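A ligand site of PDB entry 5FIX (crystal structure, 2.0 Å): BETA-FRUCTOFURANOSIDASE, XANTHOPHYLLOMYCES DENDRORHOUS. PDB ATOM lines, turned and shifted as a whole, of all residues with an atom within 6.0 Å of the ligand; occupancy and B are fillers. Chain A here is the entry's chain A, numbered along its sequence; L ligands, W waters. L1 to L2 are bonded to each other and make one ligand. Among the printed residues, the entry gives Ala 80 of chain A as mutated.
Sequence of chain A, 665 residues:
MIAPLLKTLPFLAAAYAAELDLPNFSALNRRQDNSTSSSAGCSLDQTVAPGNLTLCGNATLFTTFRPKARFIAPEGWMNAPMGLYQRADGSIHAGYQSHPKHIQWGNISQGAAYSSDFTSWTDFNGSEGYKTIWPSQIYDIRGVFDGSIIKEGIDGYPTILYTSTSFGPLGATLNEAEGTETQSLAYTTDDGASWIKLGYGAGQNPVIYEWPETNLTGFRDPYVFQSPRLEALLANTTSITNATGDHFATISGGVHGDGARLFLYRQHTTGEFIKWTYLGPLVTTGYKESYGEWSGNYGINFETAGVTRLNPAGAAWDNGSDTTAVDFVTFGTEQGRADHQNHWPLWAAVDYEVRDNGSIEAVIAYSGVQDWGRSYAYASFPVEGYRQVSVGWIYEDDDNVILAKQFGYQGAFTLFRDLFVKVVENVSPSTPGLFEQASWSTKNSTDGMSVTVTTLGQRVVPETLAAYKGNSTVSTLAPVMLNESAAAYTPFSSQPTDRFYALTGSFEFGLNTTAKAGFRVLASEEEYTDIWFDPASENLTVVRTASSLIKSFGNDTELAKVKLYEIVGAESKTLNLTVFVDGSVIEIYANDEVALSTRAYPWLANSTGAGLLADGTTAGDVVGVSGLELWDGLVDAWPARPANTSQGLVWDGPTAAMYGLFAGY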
ATOM      1  N   ASN A  79     -31.540  -8.063 -21.935  1.00  0.00           N
ATOM      2  CA  ASN A  79     -30.498  -8.438 -21.000  1.00  0.00           C
ATOM      3  C   ASN A  79     -31.000  -9.507 -20.007  1.00  0.00           C
ATOM      4  O   ASN A  79     -31.393 -10.589 -20.465  1.00  0.00           O
ATOM      5  CB  ASN A  79     -29.731  -7.207 -20.391  1.00  0.00           C
ATOM      6  CG  ASN A  79     -30.601  -6.186 -19.661  1.00  0.00           C
ATOM      7  OD1 ASN A  79     -31.445  -5.517 -20.254  1.00  0.00           O
ATOM      8  ND2 ASN A  79     -30.353  -6.027 -18.364  1.00  0.00           N
ATOM      9  N   ALA A  80     -30.986  -9.239 -18.705  1.00  0.00           N
ATOM     10  CA  ALA A  80     -31.166 -10.247 -17.658  1.00  0.00           C
ATOM     11  C   ALA A  80     -32.466 -11.051 -17.773  1.00  0.00           C
ATOM     12  O   ALA A  80     -33.525 -10.482 -17.996  1.00  0.00           O
ATOM     13  CB  ALA A  80     -31.136  -9.568 -16.301  1.00  0.00           C
ATOM     14  N   GLN A  97     -35.408  -8.798 -19.306  1.00  0.00           N
ATOM     15  CA  GLN A  97     -35.264  -7.373 -19.481  1.00  0.00           C
ATOM     16  C   GLN A  97     -35.236  -7.083 -21.013  1.00  0.00           C
ATOM     17  O   GLN A  97     -34.429  -7.686 -21.725  1.00  0.00           O
ATOM     18  CB  GLN A  97     -33.970  -6.895 -18.826  1.00  0.00           C
ATOM     19  CG  GLN A  97     -33.991  -7.013 -17.315  1.00  0.00           C
ATOM     20  CD  GLN A  97     -34.763  -5.896 -16.663  1.00  0.00           C
ATOM     21  OE1 GLN A  97     -34.196  -4.828 -16.395  1.00  0.00           O
ATOM     22  NE2 GLN A  97     -36.044  -6.136 -16.364  1.00  0.00           N
ATOM     23  N   TRP A 105     -30.048  -0.388 -24.058  1.00  0.00           N
ATOM     24  CA  TRP A 105     -30.950  -0.476 -22.911  1.00  0.00           C
ATOM     25  C   TRP A 105     -31.813   0.785 -22.735  1.00  0.00           C
ATOM     26  O   TRP A 105     -31.378   1.893 -23.039  1.00  0.00           O
ATOM     27  CB  TRP A 105     -30.083  -0.724 -21.670  1.00  0.00           C
ATOM     28  CG  TRP A 105     -30.738  -0.903 -20.328  1.00  0.00           C
ATOM     29  CD1 TRP A 105     -31.012  -2.079 -19.705  1.00  0.00           C
ATOM     30  CD2 TRP A 105     -31.093   0.134 -19.412  1.00  0.00           C
ATOM     31  NE1 TRP A 105     -31.566  -1.845 -18.471  1.00  0.00           N
ATOM     32  CE2 TRP A 105     -31.604  -0.486 -18.259  1.00  0.00           C
ATOM     33  CE3 TRP A 105     -31.023   1.541 -19.455  1.00  0.00           C
ATOM     34  CZ2 TRP A 105     -32.057   0.230 -17.153  1.00  0.00           C
ATOM     35  CZ3 TRP A 105     -31.460   2.256 -18.355  1.00  0.00           C
ATOM     36  CH2 TRP A 105     -31.971   1.609 -17.217  1.00  0.00           C
ATOM     37  N   ILE A 108     -36.915  -0.085 -19.527  1.00  0.00           N
ATOM     38  CA  ILE A 108     -36.686  -1.519 -19.475  1.00  0.00           C
ATOM     39  C   ILE A 108     -37.963  -2.204 -18.963  1.00  0.00           C
ATOM     40  O   ILE A 108     -38.594  -1.724 -18.022  1.00  0.00           O
ATOM     41  CB  ILE A 108     -35.376  -1.882 -18.747  1.00  0.00           C
ATOM     42  CG1 ILE A 108     -34.825  -3.236 -19.236  1.00  0.00           C
ATOM     43  CG2 ILE A 108     -35.535  -1.863 -17.226  1.00  0.00           C
ATOM     44  CD1 ILE A 108     -34.310  -3.241 -20.678  1.00  0.00           C
ATOM     45  N   VAL A 144     -38.750  -1.122 -15.256  1.00  0.00           N
ATOM     46  CA  VAL A 144     -39.117  -2.333 -14.573  1.00  0.00           C
ATOM     47  C   VAL A 144     -37.900  -3.256 -14.615  1.00  0.00           C
ATOM     48  O   VAL A 144     -37.670  -3.971 -15.603  1.00  0.00           O
ATOM     49  CB  VAL A 144     -40.351  -3.001 -15.241  1.00  0.00           C
ATOM     50  CG1 VAL A 144     -40.648  -4.362 -14.625  1.00  0.00           C
ATOM     51  CG2 VAL A 144     -41.550  -2.087 -15.109  1.00  0.00           C
ATOM     52  N   PHE A 145     -37.115  -3.217 -13.544  1.00  0.00           N
ATOM     53  CA  PHE A 145     -35.861  -3.962 -13.425  1.00  0.00           C
ATOM     54  C   PHE A 145     -36.177  -5.418 -13.025  1.00  0.00           C
ATOM     55  O   PHE A 145     -37.333  -5.845 -13.058  1.00  0.00           O
ATOM     56  CB  PHE A 145     -34.931  -3.286 -12.388  1.00  0.00           C
ATOM     57  CG  PHE A 145     -34.199  -2.062 -12.892  1.00  0.00           C
ATOM     58  CD1 PHE A 145     -34.702  -1.232 -13.878  1.00  0.00           C
ATOM     59  CD2 PHE A 145     -32.996  -1.707 -12.279  1.00  0.00           C
ATOM     60  CE1 PHE A 145     -34.027  -0.089 -14.277  1.00  0.00           C
ATOM     61  CE2 PHE A 145     -32.300  -0.562 -12.670  1.00  0.00           C
ATOM     62  CZ  PHE A 145     -32.817   0.245 -13.676  1.00  0.00           C
ATOM     63  N   ASP A 146     -35.132  -6.197 -12.736  1.00  0.00           N
ATOM     64  CA  ASP A 146     -35.242  -7.627 -12.401  1.00  0.00           C
ATOM     65  C   ASP A 146     -36.207  -7.878 -11.239  1.00  0.00           C
ATOM     66  O   ASP A 146     -36.373  -7.041 -10.348  1.00  0.00           O
ATOM     67  CB  ASP A 146     -33.839  -8.127 -12.040  1.00  0.00           C
ATOM     68  CG  ASP A 146     -33.724  -9.648 -11.945  1.00  0.00           C
ATOM     69  OD1 ASP A 146     -34.579 -10.414 -12.438  1.00  0.00           O
ATOM     70  OD2 ASP A 146     -32.695 -10.084 -11.345  1.00  0.00           O
ATOM     71  N   THR A 163     -37.819  -4.796  -8.989  1.00  0.00           N
ATOM     72  CA  THR A 163     -37.295  -3.467  -8.711  1.00  0.00           C
ATOM     73  C   THR A 163     -37.959  -2.427  -9.607  1.00  0.00           C
ATOM     74  O   THR A 163     -37.812  -2.452 -10.834  1.00  0.00           O
ATOM     75  CB  THR A 163     -35.778  -3.408  -8.824  1.00  0.00           C
ATOM     76  OG1 THR A 163     -35.189  -4.290  -7.861  1.00  0.00           O
ATOM     77  CG2 THR A 163     -35.285  -1.995  -8.606  1.00  0.00           C
ATOM     78  N   LEU A 170     -28.587   6.724 -10.688  1.00  0.00           N
ATOM     79  CA  LEU A 170     -28.750   5.315 -10.410  1.00  0.00           C
ATOM     80  C   LEU A 170     -27.481   4.611 -10.898  1.00  0.00           C
ATOM     81  O   LEU A 170     -27.162   4.656 -12.098  1.00  0.00           O
ATOM     82  CB  LEU A 170     -29.998   4.780 -11.134  1.00  0.00           C
ATOM     83  CG  LEU A 170     -30.564   3.399 -10.697  1.00  0.00           C
ATOM     84  CD1 LEU A 170     -31.954   3.185 -11.285  1.00  0.00           C
ATOM     85  CD2 LEU A 170     -29.642   2.250 -11.090  1.00  0.00           C
ATOM     86  N   GLY A 171     -26.753   4.001  -9.970  1.00  0.00           N
ATOM     87  CA  GLY A 171     -25.571   3.234 -10.317  1.00  0.00           C
ATOM     88  C   GLY A 171     -24.587   3.155  -9.189  1.00  0.00           C
ATOM     89  O   GLY A 171     -24.514   4.053  -8.347  1.00  0.00           O
ATOM     90  N   ALA A 172     -23.799   2.080  -9.198  1.00  0.00           N
ATOM     91  CA  ALA A 172     -22.835   1.802  -8.154  1.00  0.00           C
ATOM     92  C   ALA A 172     -21.709   2.838  -8.068  1.00  0.00           C
ATOM     93  O   ALA A 172     -21.145   3.042  -6.989  1.00  0.00           O
ATOM     94  CB  ALA A 172     -22.255   0.409  -8.362  1.00  0.00           C
ATOM     95  N   ARG A 220     -31.489  -3.497  -5.439  1.00  0.00           N
ATOM     96  CA  ARG A 220     -32.306  -4.085  -6.487  1.00  0.00           C
ATOM     97  C   ARG A 220     -32.218  -5.598  -6.603  1.00  0.00           C
ATOM     98  O   ARG A 220     -31.432  -6.240  -5.896  1.00  0.00           O
ATOM     99  CB  ARG A 220     -31.923  -3.451  -7.841  1.00  0.00           C
ATOM    100  CG  ARG A 220     -30.480  -3.627  -8.287  1.00  0.00           C
ATOM    101  CD  ARG A 220     -30.298  -3.181  -9.741  1.00  0.00           C
ATOM    102  NE  ARG A 220     -28.891  -3.027 -10.098  1.00  0.00           N
ATOM    103  CZ  ARG A 220     -28.119  -1.998  -9.736  1.00  0.00           C
ATOM    104  NH1 ARG A 220     -28.613  -0.980  -9.030  1.00  0.00           N
ATOM    105  NH2 ARG A 220     -26.841  -1.978 -10.064  1.00  0.00           N
ATOM    106  N   ASP A 221     -33.042  -6.123  -7.504  1.00  0.00           N
ATOM    107  CA  ASP A 221     -33.044  -7.518  -7.917  1.00  0.00           C
ATOM    108  C   ASP A 221     -33.520  -8.431  -6.792  1.00  0.00           C
ATOM    109  O   ASP A 221     -32.798  -9.361  -6.392  1.00  0.00           O
ATOM    110  CB  ASP A 221     -31.675  -7.954  -8.465  1.00  0.00           C
ATOM    111  CG  ASP A 221     -31.161  -7.040  -9.588  1.00  0.00           C
ATOM    112  OD1 ASP A 221     -31.983  -6.295 -10.171  1.00  0.00           O
ATOM    113  OD2 ASP A 221     -29.947  -7.071  -9.839  1.00  0.00           O
ATOM    114  N   PHE A 302     -23.230  -5.934  -5.579  1.00  0.00           N
ATOM    115  CA  PHE A 302     -23.844  -7.178  -6.074  1.00  0.00           C
ATOM    116  C   PHE A 302     -25.056  -6.863  -6.917  1.00  0.00           C
ATOM    117  O   PHE A 302     -25.733  -5.862  -6.724  1.00  0.00           O
ATOM    118  CB  PHE A 302     -24.326  -8.106  -4.943  1.00  0.00           C
ATOM    119  CG  PHE A 302     -23.226  -8.762  -4.134  1.00  0.00           C
ATOM    120  CD1 PHE A 302     -21.991  -9.095  -4.687  1.00  0.00           C
ATOM    121  CD2 PHE A 302     -23.475  -9.102  -2.812  1.00  0.00           C
ATOM    122  CE1 PHE A 302     -21.012  -9.712  -3.900  1.00  0.00           C
ATOM    123  CE2 PHE A 302     -22.503  -9.725  -2.029  1.00  0.00           C
ATOM    124  CZ  PHE A 302     -21.279 -10.041  -2.582  1.00  0.00           C
ATOM    125  N   GLU A 303     -25.340  -7.775  -7.843  1.00  0.00           N
ATOM    126  CA  GLU A 303     -26.530  -7.734  -8.661  1.00  0.00           C
ATOM    127  C   GLU A 303     -27.052  -9.143  -8.878  1.00  0.00           C
ATOM    128  O   GLU A 303     -26.291 -10.111  -8.791  1.00  0.00           O
ATOM    129  CB  GLU A 303     -26.225  -7.105 -10.032  1.00  0.00           C
ATOM    130  CG  GLU A 303     -25.657  -5.697  -9.972  1.00  0.00           C
ATOM    131  CD  GLU A 303     -25.387  -5.141 -11.356  1.00  0.00           C
ATOM    132  OE1 GLU A 303     -24.633  -5.759 -12.130  1.00  0.00           O
ATOM    133  OE2 GLU A 303     -25.899  -4.053 -11.659  1.00  0.00           O
ATOM    134  N   THR A 304     -28.341  -9.226  -9.173  1.00  0.00           N
ATOM    135  CA  THR A 304     -29.060 -10.460  -9.510  1.00  0.00           C
ATOM    136  C   THR A 304     -28.709 -11.637  -8.603  1.00  0.00           C
ATOM    137  O   THR A 304     -28.595 -12.752  -9.069  1.00  0.00           O
ATOM    138  CB  THR A 304     -28.913 -10.871 -11.007  1.00  0.00           C
ATOM    139  OG1 THR A 304     -27.610 -11.444 -11.258  1.00  0.00           O
ATOM    140  CG2 THR A 304     -29.137  -9.694 -11.936  1.00  0.00           C
ATOM    141  N   GLU A 334     -19.923  -6.071  -9.701  1.00  0.00           N
ATOM    142  CA  GLU A 334     -19.570  -4.963 -10.566  1.00  0.00           C
ATOM    143  C   GLU A 334     -18.263  -4.294 -10.119  1.00  0.00           C
ATOM    144  O   GLU A 334     -18.003  -4.179  -8.923  1.00  0.00           O
ATOM    145  CB  GLU A 334     -20.619  -3.855 -10.489  1.00  0.00           C
ATOM    146  CG  GLU A 334     -22.071  -4.280 -10.621  1.00  0.00           C
ATOM    147  CD  GLU A 334     -22.908  -3.105 -11.082  1.00  0.00           C
ATOM    148  OE1 GLU A 334     -22.919  -2.862 -12.315  1.00  0.00           O
ATOM    149  OE2 GLU A 334     -23.506  -2.438 -10.215  1.00  0.00           O
ATOM    150  N   HIS A 343     -17.960  -7.100 -15.079  1.00  0.00           N
ATOM    151  CA  HIS A 343     -18.963  -7.995 -14.479  1.00  0.00           C
ATOM    152  C   HIS A 343     -18.486  -9.437 -14.303  1.00  0.00           C
ATOM    153  O   HIS A 343     -18.079 -10.081 -15.272  1.00  0.00           O
ATOM    154  CB  HIS A 343     -20.197  -8.024 -15.378  1.00  0.00           C
ATOM    155  CG  HIS A 343     -21.151  -6.903 -15.129  1.00  0.00           C
ATOM    156  ND1 HIS A 343     -22.010  -6.431 -16.103  1.00  0.00           N
ATOM    157  CD2 HIS A 343     -21.397  -6.145 -14.032  1.00  0.00           C
ATOM    158  CE1 HIS A 343     -22.743  -5.452 -15.612  1.00  0.00           C
ATOM    159  NE2 HIS A 343     -22.394  -5.263 -14.351  1.00  0.00           N
ATOM    160  N   TYR A 376     -23.693 -13.006 -17.807  1.00  0.00           N
ATOM    161  CA  TYR A 376     -23.971 -12.322 -16.552  1.00  0.00           C
ATOM    162  C   TYR A 376     -25.454 -12.479 -16.221  1.00  0.00           C
ATOM    163  O   TYR A 376     -26.225 -12.941 -17.050  1.00  0.00           O
ATOM    164  CB  TYR A 376     -23.638 -10.840 -16.686  1.00  0.00           C
ATOM    165  CG  TYR A 376     -23.541 -10.071 -15.387  1.00  0.00           C
ATOM    166  CD1 TYR A 376     -22.600 -10.392 -14.423  1.00  0.00           C
ATOM    167  CD2 TYR A 376     -24.385  -8.985 -15.129  1.00  0.00           C
ATOM    168  CE1 TYR A 376     -22.487  -9.679 -13.246  1.00  0.00           C
ATOM    169  CE2 TYR A 376     -24.293  -8.262 -13.947  1.00  0.00           C
ATOM    170  CZ  TYR A 376     -23.333  -8.595 -13.010  1.00  0.00           C
ATOM    171  OH  TYR A 376     -23.205  -7.896 -11.841  1.00  0.00           O
ATOM    172  N   ALA A 377     -25.819 -12.096 -15.004  1.00  0.00           N
ATOM    173  CA  ALA A 377     -27.220 -11.978 -14.587  1.00  0.00           C
ATOM    174  C   ALA A 377     -27.882 -13.324 -14.593  1.00  0.00           C
ATOM    175  O   ALA A 377     -28.980 -13.484 -15.106  1.00  0.00           O
ATOM    176  CB  ALA A 377     -27.972 -10.972 -15.465  1.00  0.00           C
ATOM    177  N   TRP A 393     -27.571 -14.432 -19.159  1.00  0.00           N
ATOM    178  CA  TRP A 393     -27.619 -13.596 -20.355  1.00  0.00           C
ATOM    179  C   TRP A 393     -26.239 -13.534 -20.973  1.00  0.00           C
ATOM    180  O   TRP A 393     -25.274 -13.250 -20.270  1.00  0.00           O
ATOM    181  CB  TRP A 393     -28.104 -12.203 -19.955  1.00  0.00           C
ATOM    182  CG  TRP A 393     -27.714 -11.035 -20.851  1.00  0.00           C
ATOM    183  CD1 TRP A 393     -28.052 -10.833 -22.158  1.00  0.00           C
ATOM    184  CD2 TRP A 393     -26.991  -9.867 -20.449  1.00  0.00           C
ATOM    185  NE1 TRP A 393     -27.555  -9.643 -22.608  1.00  0.00           N
ATOM    186  CE2 TRP A 393     -26.906  -9.024 -21.578  1.00  0.00           C
ATOM    187  CE3 TRP A 393     -26.396  -9.469 -19.251  1.00  0.00           C
ATOM    188  CZ2 TRP A 393     -26.252  -7.788 -21.530  1.00  0.00           C
ATOM    189  CZ3 TRP A 393     -25.744  -8.247 -19.206  1.00  0.00           C
ATOM    190  CH2 TRP A 393     -25.669  -7.422 -20.341  1.00  0.00           C
HETATM  191  C1  LIG L   1     -27.669  -3.425 -15.091  1.00  0.00           C
HETATM  192  C2  LIG L   1     -26.187  -3.047 -14.872  1.00  0.00           C
HETATM  193  C3  LIG L   1     -26.039  -1.956 -13.832  1.00  0.00           C
HETATM  194  C4  LIG L   1     -26.902  -0.769 -14.171  1.00  0.00           C
HETATM  195  C5  LIG L   1     -28.347  -1.214 -14.315  1.00  0.00           C
HETATM  196  C6  LIG L   1     -29.245  -0.066 -14.747  1.00  0.00           C
HETATM  197  O1  LIG L   1     -25.414  -4.184 -14.469  1.00  0.00           O
HETATM  198  O2  LIG L   1     -24.667  -1.575 -13.745  1.00  0.00           O
HETATM  199  O3  LIG L   1     -26.789   0.203 -13.131  1.00  0.00           O
HETATM  200  O4  LIG L   1     -28.457  -2.252 -15.290  1.00  0.00           O
HETATM  201  O5  LIG L   1     -28.768   0.492 -15.987  1.00  0.00           O
HETATM  202  C1  LG2 L   2     -27.821  -6.582 -14.290  1.00  0.00           C
HETATM  203  C2  LG2 L   2     -28.830  -5.431 -14.139  1.00  0.00           C
HETATM  204  C3  LG2 L   2     -29.723  -5.740 -12.931  1.00  0.00           C
HETATM  205  C4  LG2 L   2     -30.921  -4.858 -13.211  1.00  0.00           C
HETATM  206  C5  LG2 L   2     -31.046  -4.994 -14.730  1.00  0.00           C
HETATM  207  C6  LG2 L   2     -31.545  -3.725 -15.424  1.00  0.00           C
HETATM  208  O1  LG2 L   2     -26.833  -6.308 -15.280  1.00  0.00           O
HETATM  209  O2  LG2 L   2     -28.208  -4.139 -13.963  1.00  0.00           O
HETATM  210  O3  LG2 L   2     -29.073  -5.518 -11.671  1.00  0.00           O
HETATM  211  O4  LG2 L   2     -32.123  -5.280 -12.553  1.00  0.00           O
HETATM  212  O5  LG2 L   2     -29.767  -5.402 -15.206  1.00  0.00           O
HETATM  213  O6  LG2 L   2     -31.865  -4.009 -16.799  1.00  0.00           O
HETATM  214  O   HOH W   1     -27.936  -1.129 -18.319  1.00  0.00           O
HETATM  215  O   HOH W   2     -28.812   3.153 -16.149  1.00  0.00           O
HETATM  216  O   HOH W   3     -28.119  -7.450 -17.254  1.00  0.00           O
HETATM  217  O   HOH W   4     -23.555   0.469 -15.220  1.00  0.00           O
HETATM  218  O   HOH W   5     -26.863   2.691 -13.931  1.00  0.00           O
HETATM  219  O   HOH W   6     -24.593  -0.122 -11.010  1.00  0.00           O
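Residues that only touch the ligand: Ile 108 (3.9 Å), Phe 145 (3.4 Å) and Tyr 376 (3.5 Å). Hydrophobic or aromatic side chains within 4 Å of the ligand: Trp 105, Ile 108, Phe 145, His 343 and Tyr 376. Along chain A the residues within 4 Å of the ligand span positions 79 to 376.
NE2 of Gln 97 is in hydrogen-bond range of O of Val 144, at 2.8 Å. O of Asp 146 sits at hydrogen-bond distance from N of Thr 163, at 3.0 Å. The backbone NH (N) of Gln 97 sits at hydrogen-bond distance from the backbone carbonyl oxygen (O) of Ala 80, at 2.8 Å. N of Asn 79 sits at hydrogen-bond distance from O of Gln 97 (2.9 Å). NH2 of Arg 220 lies within salt-bridge range of OE2 of Glu 303 (2.8 Å). The side-chain carboxylate (OE1) of Glu 334 lies within hydrogen-bond range of a ring nitrogen (NE2) of His 343, at 3.2 Å. The backbone carbonyl oxygen (O) of Tyr 376 lies within hydrogen-bond range of the backbone NH (N) of Trp 393, 2.9 Å away. OE1 of Glu 303 sits at hydrogen-bond distance from OH of Tyr 376, 2.6 Å away.
Water W5 lies within hydrogen-bond range of O3 of LIG L1 (2.6 Å) and O of Leu 170 (2.7 Å). Water W3 lies within hydrogen-bond range of O1 of LG2 L2 (2.6 Å) and ND2 of Asn 79 (2.9 Å). Water W6 lies within hydrogen-bond range of the side-chain carboxylate of Glu 334, the backbone NH of Ala 172, the guanidinium group of Arg 220 and an oxygen (O3) of LIG L1.
The indole nitrogen (NE1) of Trp 105 sits at hydrogen-bond distance from an oxygen (O6) of LG2 L2 (2.8 Å). The side-chain amide nitrogen of Asn 79 is in hydrogen-bond range of an oxygen (O6) of LG2 L2, 3.0 Å away. A ring nitrogen (NE2) of His 343 sits close to an oxygen (O1) of LIG L1 (3.2 Å). OE1 of Glu 334 is in hydrogen-bond range of O2 of LIG L1 (2.6 Å). The backbone NH (N) of Asp 146 lies within hydrogen-bond range of an oxygen (O4) of LG2 L2 (3.2 Å). OE2 of Glu 303 sits at hydrogen-bond distance from O1 of LIG L1, at 2.9 Å. The side-chain amide oxygen of Gln 97 is in hydrogen-bond range of an oxygen (O6) of LG2 L2. The side-chain carboxylate (OD2) of Asp 221 lies within hydrogen-bond range of an oxygen (O3) of LG2 L2. An oxygen (O3) of LG2 L2 lies within hydrogen-bond range of the guanidinium group (NE) of Arg 220 (3.0 Å).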
